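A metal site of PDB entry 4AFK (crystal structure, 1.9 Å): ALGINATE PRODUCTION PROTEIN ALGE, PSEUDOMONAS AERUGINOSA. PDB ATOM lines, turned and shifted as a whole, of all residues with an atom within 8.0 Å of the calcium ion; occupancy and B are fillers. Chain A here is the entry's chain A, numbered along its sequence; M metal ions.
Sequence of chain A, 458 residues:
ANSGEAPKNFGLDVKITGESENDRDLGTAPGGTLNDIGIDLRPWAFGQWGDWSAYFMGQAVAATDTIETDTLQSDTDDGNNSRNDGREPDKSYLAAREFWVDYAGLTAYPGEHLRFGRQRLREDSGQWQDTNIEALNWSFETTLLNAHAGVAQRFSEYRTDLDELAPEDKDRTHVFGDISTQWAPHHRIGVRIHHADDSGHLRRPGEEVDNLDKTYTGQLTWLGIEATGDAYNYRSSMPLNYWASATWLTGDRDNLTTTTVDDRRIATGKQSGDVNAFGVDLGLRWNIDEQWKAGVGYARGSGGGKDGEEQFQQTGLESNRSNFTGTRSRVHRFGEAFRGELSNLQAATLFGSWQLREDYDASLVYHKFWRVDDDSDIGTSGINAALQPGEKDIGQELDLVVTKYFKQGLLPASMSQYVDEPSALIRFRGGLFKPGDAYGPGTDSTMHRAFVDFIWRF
The backbone NH of Gly 27 lies close to the side-chain carboxylate of Asp 23 (3.2 Å).
The side-chain carboxylate (OD1) of Asp 25 sits close to the backbone NH (N) of Gly 27.
The backbone carbonyl oxygen of Asp 25 sits at hydrogen-bond distance from the side-chain hydroxyl of Thr 28.
Merely in contact with the calcium ion: Pro 30 (3.7 Å).
Of the 14 residues printed, 5 come within 4 Å of the calcium ion.
The nearest printed residue that does not touch the calcium ion is Gly 27 (4.4 Å).
The calcium ion is bound by the backbone carbonyl oxygen of Gly 31 (2.5 Å), the side-chain carboxylate of Asp 23 (2.5 Å), the backbone carbonyl oxygen of Ala 29 (2.6 Å) and the side-chain carboxylate of Asp 25 (2.8 Å).
Slightly farther from the calcium ion lies OD1 of Asp 23 (3.0 Å).
Slightly farther from the calcium ion lies OD2 of Asp 25 (3.0 Å).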
ATOM      1  N   ASN A  22      -6.158 -23.393  16.711  1.00  0.00           N
ATOM      2  CA  ASN A  22      -6.635 -24.125  17.878  1.00  0.00           C
ATOM      3  C   ASN A  22      -7.403 -25.329  17.376  1.00  0.00           C
ATOM      4  O   ASN A  22      -8.485 -25.159  16.828  1.00  0.00           O
ATOM      5  CB  ASN A  22      -7.575 -23.220  18.684  1.00  0.00           C
ATOM      6  CG  ASN A  22      -7.743 -23.672  20.121  1.00  0.00           C
ATOM      7  OD1 ASN A  22      -7.848 -24.854  20.406  1.00  0.00           O
ATOM      8  ND2 ASN A  22      -7.761 -22.703  21.039  1.00  0.00           N
ATOM      9  N   ASP A  23      -6.895 -26.539  17.547  1.00  0.00           N
ATOM     10  CA  ASP A  23      -5.612 -26.846  18.157  1.00  0.00           C
ATOM     11  C   ASP A  23      -4.930 -27.800  17.164  1.00  0.00           C
ATOM     12  O   ASP A  23      -5.494 -28.831  16.792  1.00  0.00           O
ATOM     13  CB  ASP A  23      -5.866 -27.527  19.495  1.00  0.00           C
ATOM     14  CG  ASP A  23      -4.627 -28.081  20.142  1.00  0.00           C
ATOM     15  OD1 ASP A  23      -3.526 -28.127  19.519  1.00  0.00           O
ATOM     16  OD2 ASP A  23      -4.768 -28.467  21.315  1.00  0.00           O
ATOM     17  N   ARG A  24      -3.732 -27.443  16.737  1.00  0.00           N
ATOM     18  CA  ARG A  24      -3.039 -28.169  15.685  1.00  0.00           C
ATOM     19  C   ARG A  24      -2.920 -29.670  15.993  1.00  0.00           C
ATOM     20  O   ARG A  24      -2.960 -30.520  15.090  1.00  0.00           O
ATOM     21  CB  ARG A  24      -1.649 -27.561  15.494  1.00  0.00           C
ATOM     22  CG  ARG A  24      -0.915 -28.041  14.283  1.00  0.00           C
ATOM     23  CD  ARG A  24       0.464 -27.414  14.211  1.00  0.00           C
ATOM     24  NE  ARG A  24       1.114 -27.716  12.936  1.00  0.00           N
ATOM     25  CZ  ARG A  24       1.316 -26.825  11.977  1.00  0.00           C
ATOM     26  NH1 ARG A  24       0.931 -25.562  12.144  1.00  0.00           N
ATOM     27  NH2 ARG A  24       1.907 -27.204  10.857  1.00  0.00           N
ATOM     28  N   ASP A  25      -2.779 -30.005  17.267  1.00  0.00           N
ATOM     29  CA  ASP A  25      -2.686 -31.420  17.619  1.00  0.00           C
ATOM     30  C   ASP A  25      -3.988 -32.008  18.154  1.00  0.00           C
ATOM     31  O   ASP A  25      -3.998 -33.095  18.726  1.00  0.00           O
ATOM     32  CB  ASP A  25      -1.498 -31.692  18.553  1.00  0.00           C
ATOM     33  CG  ASP A  25      -1.596 -30.954  19.850  1.00  0.00           C
ATOM     34  OD1 ASP A  25      -2.640 -31.068  20.520  1.00  0.00           O
ATOM     35  OD2 ASP A  25      -0.620 -30.246  20.197  1.00  0.00           O
ATOM     36  N   LEU A  26      -5.082 -31.269  17.967  1.00  0.00           N
ATOM     37  CA  LEU A  26      -6.428 -31.773  18.305  1.00  0.00           C
ATOM     38  C   LEU A  26      -6.610 -32.093  19.785  1.00  0.00           C
ATOM     39  O   LEU A  26      -7.446 -32.936  20.163  1.00  0.00           O
ATOM     40  CB  LEU A  26      -6.758 -33.007  17.443  1.00  0.00           C
ATOM     41  CG  LEU A  26      -6.681 -32.844  15.922  1.00  0.00           C
ATOM     42  CD1 LEU A  26      -7.315 -34.104  15.274  1.00  0.00           C
ATOM     43  CD2 LEU A  26      -7.415 -31.575  15.504  1.00  0.00           C
ATOM     44  N   GLY A  27      -5.826 -31.418  20.634  1.00  0.00           N
ATOM     45  CA  GLY A  27      -5.947 -31.604  22.070  1.00  0.00           C
ATOM     46  C   GLY A  27      -5.098 -32.735  22.612  1.00  0.00           C
ATOM     47  O   GLY A  27      -5.176 -33.048  23.796  1.00  0.00           O
ATOM     48  N   THR A  28      -4.269 -33.346  21.760  1.00  0.00           N
ATOM     49  CA  THR A  28      -3.509 -34.511  22.190  1.00  0.00           C
ATOM     50  C   THR A  28      -2.261 -34.172  23.010  1.00  0.00           C
ATOM     51  O   THR A  28      -1.869 -34.937  23.892  1.00  0.00           O
ATOM     52  CB  THR A  28      -3.163 -35.470  21.015  1.00  0.00           C
ATOM     53  OG1 THR A  28      -2.395 -34.790  20.017  1.00  0.00           O
ATOM     54  CG2 THR A  28      -4.437 -35.997  20.368  1.00  0.00           C
ATOM     55  N   ALA A  29      -1.652 -33.026  22.733  1.00  0.00           N
ATOM     56  CA  ALA A  29      -0.461 -32.582  23.460  1.00  0.00           C
ATOM     57  C   ALA A  29      -0.788 -31.283  24.201  1.00  0.00           C
ATOM     58  O   ALA A  29      -1.849 -30.716  23.981  1.00  0.00           O
ATOM     59  CB  ALA A  29       0.705 -32.387  22.492  1.00  0.00           C
ATOM     60  N   PRO A  30       0.120 -30.821  25.075  1.00  0.00           N
ATOM     61  CA  PRO A  30      -0.148 -29.611  25.881  1.00  0.00           C
ATOM     62  C   PRO A  30      -0.055 -28.316  25.074  1.00  0.00           C
ATOM     63  O   PRO A  30       0.666 -28.282  24.071  1.00  0.00           O
ATOM     64  CB  PRO A  30       0.964 -29.638  26.948  1.00  0.00           C
ATOM     65  CG  PRO A  30       1.532 -31.025  26.912  1.00  0.00           C
ATOM     66  CD  PRO A  30       1.380 -31.478  25.490  1.00  0.00           C
ATOM     67  N   GLY A  31      -0.737 -27.270  25.534  1.00  0.00           N
ATOM     68  CA  GLY A  31      -0.674 -25.956  24.901  1.00  0.00           C
ATOM     69  C   GLY A  31      -0.616 -25.989  23.384  1.00  0.00           C
ATOM     70  O   GLY A  31      -1.400 -26.676  22.723  1.00  0.00           O
ATOM     71  N   GLY A  32       0.307 -25.227  22.804  1.00  0.00           N
ATOM     72  CA  GLY A  32       0.520 -25.285  21.370  1.00  0.00           C
ATOM     73  C   GLY A  32      -0.631 -24.761  20.516  1.00  0.00           C
ATOM     74  O   GLY A  32      -0.893 -25.291  19.454  1.00  0.00           O
ATOM     75  N   THR A  33      -1.325 -23.733  21.007  1.00  0.00           N
ATOM     76  CA  THR A  33      -2.353 -23.045  20.241  1.00  0.00           C
ATOM     77  C   THR A  33      -1.860 -21.624  19.976  1.00  0.00           C
ATOM     78  O   THR A  33      -0.849 -21.199  20.567  1.00  0.00           O
ATOM     79  CB  THR A  33      -3.671 -22.986  21.025  1.00  0.00           C
ATOM     80  OG1 THR A  33      -3.461 -22.260  22.249  1.00  0.00           O
ATOM     81  CG2 THR A  33      -4.180 -24.393  21.374  1.00  0.00           C
ATOM     82  N   ASN A 384      -1.284 -32.171  13.627  1.00  0.00           N
ATOM     83  CA  ASN A 384      -0.244 -32.983  14.249  1.00  0.00           C
ATOM     84  C   ASN A 384      -0.830 -33.998  15.205  1.00  0.00           C
ATOM     85  O   ASN A 384      -0.809 -33.817  16.421  1.00  0.00           O
ATOM     86  CB  ASN A 384       0.720 -32.104  15.038  1.00  0.00           C
ATOM     87  CG  ASN A 384       1.518 -31.168  14.144  1.00  0.00           C
ATOM     88  OD1 ASN A 384       1.954 -30.097  14.581  1.00  0.00           O
ATOM     89  ND2 ASN A 384       1.691 -31.567  12.887  1.00  0.00           N
ATOM     90  N   ASP A 444     -10.057 -33.539  19.692  1.00  0.00           N
ATOM     91  CA  ASP A 444     -11.082 -32.504  19.530  1.00  0.00           C
ATOM     92  C   ASP A 444     -11.985 -32.809  18.350  1.00  0.00           C
ATOM     93  O   ASP A 444     -11.561 -33.432  17.380  1.00  0.00           O
ATOM     94  CB  ASP A 444     -10.428 -31.126  19.310  1.00  0.00           C
ATOM     95  CG  ASP A 444      -9.671 -30.645  20.527  1.00  0.00           C
ATOM     96  OD1 ASP A 444     -10.011 -31.073  21.653  1.00  0.00           O
ATOM     97  OD2 ASP A 444      -8.736 -29.829  20.358  1.00  0.00           O
HETATM   98 CA    CA M   1      -2.457 -28.916  22.232  1.00  0.00          CA
